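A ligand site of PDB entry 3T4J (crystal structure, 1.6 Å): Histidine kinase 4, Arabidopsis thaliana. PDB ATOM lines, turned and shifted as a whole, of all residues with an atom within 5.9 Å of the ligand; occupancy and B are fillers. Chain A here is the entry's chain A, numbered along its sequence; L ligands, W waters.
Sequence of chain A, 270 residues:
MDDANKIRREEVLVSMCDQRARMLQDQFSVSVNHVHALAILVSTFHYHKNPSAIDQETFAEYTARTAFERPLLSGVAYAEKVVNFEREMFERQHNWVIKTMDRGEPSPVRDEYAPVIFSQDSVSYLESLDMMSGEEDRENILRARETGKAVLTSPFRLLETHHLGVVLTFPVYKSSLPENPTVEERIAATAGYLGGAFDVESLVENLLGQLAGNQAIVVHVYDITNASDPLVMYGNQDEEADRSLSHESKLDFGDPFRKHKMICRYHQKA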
ATOM      1  N   SER A  74      14.605  35.468 -21.431  1.00  0.00           N
ATOM      2  CA  SER A  74      15.467  35.274 -22.588  1.00  0.00           C
ATOM      3  C   SER A  74      14.682  34.848 -23.826  1.00  0.00           C
ATOM      4  O   SER A  74      15.150  35.057 -24.948  1.00  0.00           O
ATOM      5  CB  SER A  74      16.586  34.270 -22.310  1.00  0.00           C
ATOM      6  OG  SER A  74      16.090  32.991 -22.018  1.00  0.00           O
ATOM      7  N   GLY A  75      13.501  34.267 -23.628  1.00  0.00           N
ATOM      8  CA  GLY A  75      12.697  33.780 -24.723  1.00  0.00           C
ATOM      9  C   GLY A  75      11.347  33.324 -24.202  1.00  0.00           C
ATOM     10  O   GLY A  75      11.222  33.044 -23.016  1.00  0.00           O
ATOM     11  N   ALA A  77       7.781  30.843 -25.626  1.00  0.00           N
ATOM     12  CA  ALA A  77       7.341  29.845 -26.570  1.00  0.00           C
ATOM     13  C   ALA A  77       5.951  29.340 -26.151  1.00  0.00           C
ATOM     14  O   ALA A  77       5.553  29.447 -24.974  1.00  0.00           O
ATOM     15  CB  ALA A  77       8.316  28.683 -26.618  1.00  0.00           C
ATOM     16  N   TYR A  78       5.253  28.748 -27.113  1.00  0.00           N
ATOM     17  CA  TYR A  78       3.943  28.163 -26.866  1.00  0.00           C
ATOM     18  C   TYR A  78       3.976  26.674 -27.214  1.00  0.00           C
ATOM     19  O   TYR A  78       4.329  26.283 -28.335  1.00  0.00           O
ATOM     20  CB  TYR A  78       2.852  28.855 -27.692  1.00  0.00           C
ATOM     21  CG  TYR A  78       1.513  28.232 -27.458  1.00  0.00           C
ATOM     22  CD1 TYR A  78       0.868  28.377 -26.248  1.00  0.00           C
ATOM     23  CD2 TYR A  78       0.930  27.428 -28.430  1.00  0.00           C
ATOM     24  CE1 TYR A  78      -0.359  27.739 -25.990  1.00  0.00           C
ATOM     25  CE2 TYR A  78      -0.297  26.781 -28.167  1.00  0.00           C
ATOM     26  CZ  TYR A  78      -0.920  26.946 -26.959  1.00  0.00           C
ATOM     27  OH  TYR A  78      -2.127  26.309 -26.677  1.00  0.00           O
ATOM     28  N   ALA A  79       3.601  25.880 -26.198  1.00  0.00           N
ATOM     29  CA  ALA A  79       3.537  24.418 -26.299  1.00  0.00           C
ATOM     30  C   ALA A  79       2.068  24.000 -26.314  1.00  0.00           C
ATOM     31  O   ALA A  79       1.272  24.461 -25.488  1.00  0.00           O
ATOM     32  CB  ALA A  79       4.273  23.787 -25.137  1.00  0.00           C
ATOM     33  N   MET A 101      13.469  16.434 -24.767  1.00  0.00           N
ATOM     34  CA  MET A 101      14.366  17.582 -24.599  1.00  0.00           C
ATOM     35  C   MET A 101      15.783  17.168 -24.283  1.00  0.00           C
ATOM     36  O   MET A 101      16.730  17.925 -24.527  1.00  0.00           O
ATOM     37  CB  MET A 101      13.832  18.540 -23.546  1.00  0.00           C
ATOM     38  CG  MET A 101      13.959  18.089 -22.166  1.00  0.00           C
ATOM     39  SD  MET A 101      13.577  19.457 -21.065  1.00  0.00           S
ATOM     40  CE  MET A 101      11.926  19.855 -21.630  1.00  0.00           C
ATOM     41  N   VAL A 116       6.446  22.140 -28.308  1.00  0.00           N
ATOM     42  CA  VAL A 116       6.494  23.549 -28.688  1.00  0.00           C
ATOM     43  C   VAL A 116       6.192  23.700 -30.188  1.00  0.00           C
ATOM     44  O   VAL A 116       6.850  23.079 -31.053  1.00  0.00           O
ATOM     45  CB  VAL A 116       7.818  24.171 -28.350  1.00  0.00           C
ATOM     46  CG1 VAL A 116       7.953  25.609 -29.021  1.00  0.00           C
ATOM     47  CG2 VAL A 116       7.963  24.281 -26.835  1.00  0.00           C
ATOM     48  N   VAL A 123      14.815  31.214 -28.627  1.00  0.00           N
ATOM     49  CA  VAL A 123      14.657  29.845 -28.086  1.00  0.00           C
ATOM     50  C   VAL A 123      14.138  28.903 -29.170  1.00  0.00           C
ATOM     51  O   VAL A 123      13.301  28.034 -28.916  1.00  0.00           O
ATOM     52  CB  VAL A 123      13.788  29.844 -26.829  1.00  0.00           C
ATOM     53  CG1 VAL A 123      14.524  30.511 -25.651  1.00  0.00           C
ATOM     54  CG2 VAL A 123      12.367  30.456 -27.064  1.00  0.00           C
ATOM     55  N   TYR A 125      15.480  26.492 -30.681  1.00  0.00           N
ATOM     56  CA  TYR A 125      15.816  25.100 -30.368  1.00  0.00           C
ATOM     57  C   TYR A 125      14.721  24.364 -29.606  1.00  0.00           C
ATOM     58  O   TYR A 125      14.744  23.143 -29.558  1.00  0.00           O
ATOM     59  CB  TYR A 125      17.144  25.009 -29.598  1.00  0.00           C
ATOM     60  CG  TYR A 125      17.244  25.960 -28.421  1.00  0.00           C
ATOM     61  CD1 TYR A 125      16.650  25.660 -27.200  1.00  0.00           C
ATOM     62  CD2 TYR A 125      17.937  27.162 -28.537  1.00  0.00           C
ATOM     63  CE1 TYR A 125      16.743  26.529 -26.117  1.00  0.00           C
ATOM     64  CE2 TYR A 125      18.017  28.043 -27.476  1.00  0.00           C
ATOM     65  CZ  TYR A 125      17.438  27.737 -26.267  1.00  0.00           C
ATOM     66  OH  TYR A 125      17.577  28.657 -25.257  1.00  0.00           O
ATOM     67  N   LEU A 126      13.741  25.080 -29.023  1.00  0.00           N
ATOM     68  CA  LEU A 126      12.615  24.406 -28.364  1.00  0.00           C
ATOM     69  C   LEU A 126      11.613  23.800 -29.331  1.00  0.00           C
ATOM     70  O   LEU A 126      10.822  22.946 -28.933  1.00  0.00           O
ATOM     71  CB  LEU A 126      11.858  25.354 -27.436  1.00  0.00           C
ATOM     72  CG  LEU A 126      12.600  25.985 -26.263  1.00  0.00           C
ATOM     73  CD1 LEU A 126      11.711  27.024 -25.588  1.00  0.00           C
ATOM     74  CD2 LEU A 126      13.102  24.925 -25.236  1.00  0.00           C
ATOM     75  N   MET A 131       7.767  19.564 -23.783  1.00  0.00           N
ATOM     76  CA  MET A 131       8.176  20.232 -22.562  1.00  0.00           C
ATOM     77  C   MET A 131       7.809  19.420 -21.316  1.00  0.00           C
ATOM     78  O   MET A 131       8.302  19.681 -20.228  1.00  0.00           O
ATOM     79  CB  MET A 131       7.619  21.669 -22.537  1.00  0.00           C
ATOM     80  CG  MET A 131       8.100  22.507 -23.747  1.00  0.00           C
ATOM     81  SD  MET A 131       9.862  22.477 -24.041  1.00  0.00           S
ATOM     82  CE  MET A 131      10.438  23.144 -22.476  1.00  0.00           C
ATOM     83  N   ASP A 137       9.884  21.437 -16.031  1.00  0.00           N
ATOM     84  CA  ASP A 137       8.875  21.952 -16.955  1.00  0.00           C
ATOM     85  C   ASP A 137       7.570  21.172 -16.808  1.00  0.00           C
ATOM     86  O   ASP A 137       6.483  21.765 -16.854  1.00  0.00           O
ATOM     87  CB  ASP A 137       9.388  21.895 -18.402  1.00  0.00           C
ATOM     88  CG  ASP A 137      10.278  23.083 -18.753  1.00  0.00           C
ATOM     89  OD1 ASP A 137       9.698  24.157 -18.980  1.00  0.00           O
ATOM     90  OD2 ASP A 137      11.515  22.916 -18.850  1.00  0.00           O
ATOM     91  N   ILE A 141       3.970  22.730 -15.879  1.00  0.00           N
ATOM     92  CA  ILE A 141       2.830  22.590 -16.759  1.00  0.00           C
ATOM     93  C   ILE A 141       1.607  22.105 -15.975  1.00  0.00           C
ATOM     94  O   ILE A 141       0.514  22.666 -16.108  1.00  0.00           O
ATOM     95  CB  ILE A 141       3.211  21.635 -17.927  1.00  0.00           C
ATOM     96  CG1 ILE A 141       4.025  22.445 -18.944  1.00  0.00           C
ATOM     97  CG2 ILE A 141       1.981  21.018 -18.582  1.00  0.00           C
ATOM     98  CD1 ILE A 141       4.789  21.628 -19.987  1.00  0.00           C
ATOM     99  N   PHE A 156      17.075  25.801 -12.078  1.00  0.00           N
ATOM    100  CA  PHE A 156      17.786  24.712 -12.754  1.00  0.00           C
ATOM    101  C   PHE A 156      18.478  25.230 -13.981  1.00  0.00           C
ATOM    102  O   PHE A 156      18.230  26.374 -14.398  1.00  0.00           O
ATOM    103  CB  PHE A 156      16.824  23.552 -13.107  1.00  0.00           C
ATOM    104  CG  PHE A 156      15.843  23.854 -14.208  1.00  0.00           C
ATOM    105  CD1 PHE A 156      14.778  24.719 -14.003  1.00  0.00           C
ATOM    106  CD2 PHE A 156      15.974  23.251 -15.455  1.00  0.00           C
ATOM    107  CE1 PHE A 156      13.886  24.999 -15.005  1.00  0.00           C
ATOM    108  CE2 PHE A 156      15.068  23.535 -16.475  1.00  0.00           C
ATOM    109  CZ  PHE A 156      14.024  24.394 -16.258  1.00  0.00           C
ATOM    110  N   ARG A 157      19.356  24.417 -14.564  1.00  0.00           N
ATOM    111  CA  ARG A 157      20.121  24.843 -15.721  1.00  0.00           C
ATOM    112  C   ARG A 157      19.316  24.609 -17.024  1.00  0.00           C
ATOM    113  O   ARG A 157      18.870  23.493 -17.337  1.00  0.00           O
ATOM    114  CB  ARG A 157      21.521  24.215 -15.764  1.00  0.00           C
ATOM    115  CG  ARG A 157      22.437  24.710 -14.623  1.00  0.00           C
ATOM    116  CD  ARG A 157      23.921  24.456 -14.806  1.00  0.00           C
ATOM    117  NE  ARG A 157      24.710  25.127 -13.748  1.00  0.00           N
ATOM    118  CZ  ARG A 157      25.048  26.425 -13.727  1.00  0.00           C
ATOM    119  NH1 ARG A 157      24.737  27.253 -14.730  1.00  0.00           N
ATOM    120  NH2 ARG A 157      25.740  26.899 -12.689  1.00  0.00           N
ATOM    121  N   LEU A 158      19.110  25.709 -17.727  1.00  0.00           N
ATOM    122  CA  LEU A 158      18.223  25.774 -18.866  1.00  0.00           C
ATOM    123  C   LEU A 158      18.854  25.111 -20.083  1.00  0.00           C
ATOM    124  O   LEU A 158      20.048  24.945 -20.180  1.00  0.00           O
ATOM    125  CB  LEU A 158      17.903  27.247 -19.172  1.00  0.00           C
ATOM    126  CG  LEU A 158      17.207  28.034 -18.050  1.00  0.00           C
ATOM    127  CD1 LEU A 158      16.917  29.464 -18.461  1.00  0.00           C
ATOM    128  CD2 LEU A 158      15.896  27.361 -17.624  1.00  0.00           C
ATOM    129  N   LEU A 159      18.005  24.707 -21.015  1.00  0.00           N
ATOM    130  CA  LEU A 159      18.439  24.058 -22.242  1.00  0.00           C
ATOM    131  C   LEU A 159      19.341  24.952 -23.039  1.00  0.00           C
ATOM    132  O   LEU A 159      19.175  26.167 -23.023  1.00  0.00           O
ATOM    133  CB  LEU A 159      17.207  23.691 -23.088  1.00  0.00           C
ATOM    134  CG  LEU A 159      16.411  22.496 -22.589  1.00  0.00           C
ATOM    135  CD1 LEU A 159      15.049  22.454 -23.292  1.00  0.00           C
ATOM    136  CD2 LEU A 159      17.202  21.186 -22.787  1.00  0.00           C
ATOM    137  N   VAL A 167      11.828  28.747 -14.990  1.00  0.00           N
ATOM    138  CA  VAL A 167      10.833  28.833 -16.053  1.00  0.00           C
ATOM    139  C   VAL A 167       9.499  29.296 -15.466  1.00  0.00           C
ATOM    140  O   VAL A 167       9.083  28.858 -14.370  1.00  0.00           O
ATOM    141  CB  VAL A 167      10.667  27.475 -16.755  1.00  0.00           C
ATOM    142  CG1 VAL A 167       9.417  27.461 -17.637  1.00  0.00           C
ATOM    143  CG2 VAL A 167      11.907  27.188 -17.600  1.00  0.00           C
ATOM    144  N   LEU A 168       8.857  30.171 -16.227  1.00  0.00           N
ATOM    145  CA  LEU A 168       7.527  30.723 -15.930  1.00  0.00           C
ATOM    146  C   LEU A 168       6.581  30.079 -16.925  1.00  0.00           C
ATOM    147  O   LEU A 168       6.841  30.117 -18.114  1.00  0.00           O
ATOM    148  CB  LEU A 168       7.523  32.235 -16.133  1.00  0.00           C
ATOM    149  CG  LEU A 168       6.164  32.960 -16.162  1.00  0.00           C
ATOM    150  CD1 LEU A 168       5.626  33.080 -14.748  1.00  0.00           C
ATOM    151  CD2 LEU A 168       6.268  34.365 -16.769  1.00  0.00           C
ATOM    152  N   THR A 169       5.490  29.464 -16.454  1.00  0.00           N
ATOM    153  CA  THR A 169       4.514  28.839 -17.348  1.00  0.00           C
ATOM    154  C   THR A 169       3.082  29.331 -17.023  1.00  0.00           C
ATOM    155  O   THR A 169       2.713  29.453 -15.837  1.00  0.00           O
ATOM    156  CB  THR A 169       4.619  27.306 -17.244  1.00  0.00           C
ATOM    157  OG1 THR A 169       5.979  26.889 -17.450  1.00  0.00           O
ATOM    158  CG2 THR A 169       3.696  26.611 -18.316  1.00  0.00           C
ATOM    159  N   TYR A 193       0.291  25.788 -23.233  1.00  0.00           N
ATOM    160  CA  TYR A 193       1.086  26.410 -22.205  1.00  0.00           C
ATOM    161  C   TYR A 193       2.016  27.459 -22.827  1.00  0.00           C
ATOM    162  O   TYR A 193       2.755  27.159 -23.759  1.00  0.00           O
ATOM    163  CB  TYR A 193       1.930  25.359 -21.487  1.00  0.00           C
ATOM    164  CG  TYR A 193       1.168  24.046 -21.308  1.00  0.00           C
ATOM    165  CD1 TYR A 193       0.210  23.931 -20.304  1.00  0.00           C
ATOM    166  CD2 TYR A 193       1.347  22.990 -22.182  1.00  0.00           C
ATOM    167  CE1 TYR A 193      -0.525  22.760 -20.173  1.00  0.00           C
ATOM    168  CE2 TYR A 193       0.647  21.822 -22.044  1.00  0.00           C
ATOM    169  CZ  TYR A 193      -0.310  21.722 -21.032  1.00  0.00           C
ATOM    170  OH  TYR A 193      -0.997  20.516 -20.922  1.00  0.00           O
ATOM    171  N   LEU A 194       1.984  28.679 -22.280  1.00  0.00           N
ATOM    172  CA  LEU A 194       2.874  29.753 -22.701  1.00  0.00           C
ATOM    173  C   LEU A 194       4.007  29.796 -21.660  1.00  0.00           C
ATOM    174  O   LEU A 194       3.747  30.008 -20.463  1.00  0.00           O
ATOM    175  CB  LEU A 194       2.112  31.088 -22.761  1.00  0.00           C
ATOM    176  CG  LEU A 194       2.703  32.157 -23.659  1.00  0.00           C
ATOM    177  CD1 LEU A 194       4.153  32.474 -23.316  1.00  0.00           C
ATOM    178  CD2 LEU A 194       2.607  31.789 -25.170  1.00  0.00           C
ATOM    179  N   GLY A 195       5.222  29.530 -22.088  1.00  0.00           N
ATOM    180  CA  GLY A 195       6.384  29.469 -21.184  1.00  0.00           C
ATOM    181  C   GLY A 195       7.426  30.511 -21.523  1.00  0.00           C
ATOM    182  O   GLY A 195       7.617  30.883 -22.700  1.00  0.00           O
ATOM    183  N   GLY A 196       8.090  31.001 -20.479  1.00  0.00           N
ATOM    184  CA  GLY A 196       9.167  31.963 -20.618  1.00  0.00           C
ATOM    185  C   GLY A 196      10.328  31.526 -19.770  1.00  0.00           C
ATOM    186  O   GLY A 196      10.128  30.979 -18.672  1.00  0.00           O
ATOM    187  N   ALA A 197      11.536  31.692 -20.298  1.00  0.00           N
ATOM    188  CA  ALA A 197      12.767  31.352 -19.585  1.00  0.00           C
ATOM    189  C   ALA A 197      13.341  32.595 -18.899  1.00  0.00           C
ATOM    190  O   ALA A 197      13.767  33.536 -19.576  1.00  0.00           O
ATOM    191  CB  ALA A 197      13.791  30.808 -20.556  1.00  0.00           C
HETATM  192  C1  LIG L   1       7.191  26.539 -23.542  1.00  0.00           C
HETATM  193  C2  LIG L   1       7.069  26.114 -22.108  1.00  0.00           C
HETATM  194  C3  LIG L   1       5.787  25.447 -21.669  1.00  0.00           C
HETATM  195  C4  LIG L   1       8.186  26.224 -21.158  1.00  0.00           C
HETATM  196  C5  LIG L   1       9.453  26.989 -21.472  1.00  0.00           C
HETATM  197  N1  LIG L   1      10.535  26.236 -20.901  1.00  0.00           N
HETATM  198  C6  LIG L   1      11.896  26.474 -21.273  1.00  0.00           C
HETATM  199  C7  LIG L   1      12.973  25.697 -20.793  1.00  0.00           C
HETATM  200  N2  LIG L   1      13.120  24.599 -19.982  1.00  0.00           N
HETATM  201  C8  LIG L   1      14.275  26.039 -21.210  1.00  0.00           C
HETATM  202  N3  LIG L   1      15.163  25.127 -20.680  1.00  0.00           N
HETATM  203  C9  LIG L   1      14.461  24.253 -19.938  1.00  0.00           C
HETATM  204  N4  LIG L   1      14.459  27.111 -21.980  1.00  0.00           N
HETATM  205  C10 LIG L   1      13.437  27.820 -22.456  1.00  0.00           C
HETATM  206  N5  LIG L   1      12.174  27.567 -22.060  1.00  0.00           N
HETATM  207  O   HOH W   1      16.987  27.908 -22.817  1.00  0.00           O
HETATM  208  O   HOH W   2      10.655  29.693 -23.411  1.00  0.00           O
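N of Leu 159 sits close to N3 of the ligand (2.9 Å).
A nitrogen (N2) of the ligand lies within hydrogen-bond range of the side-chain carboxylate of Asp 137 (2.6 Å).
N of Tyr 193 sits at hydrogen-bond distance from O of Ala 79, 2.8 Å away.
The backbone NH (N) of Ala 197 lies within hydrogen-bond range of the backbone carbonyl oxygen (O) of Gly 75 (3.1 Å).
The backbone NH (N) of Ser 74 sits at hydrogen-bond distance from the backbone carbonyl oxygen (O) of Ala 197 (2.8 Å).
N of Gly 195 sits at hydrogen-bond distance from O of Ala 77 (2.9 Å).
Merely in contact with the ligand: Ala 77, Leu 126, Met 131, Phe 156, Leu 158, Val 167, Tyr 193, Gly 195 and Ala 197.
Within 4 Å of the ligand: Ala 77, Leu 126, Met 131, Asp 137, Phe 156, Leu 158, Leu 159, Val 167, Tyr 193, Gly 195 and Ala 197.
The nearest printed residue that does not touch the ligand is Val 116 (4.1 Å).
Water W1 lies within hydrogen-bond range of the side-chain hydroxyl of Tyr 125 (2.6 Å), a nitrogen (N4) of the ligand (2.8 Å) and the backbone carbonyl oxygen of Leu 159 (2.8 Å).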
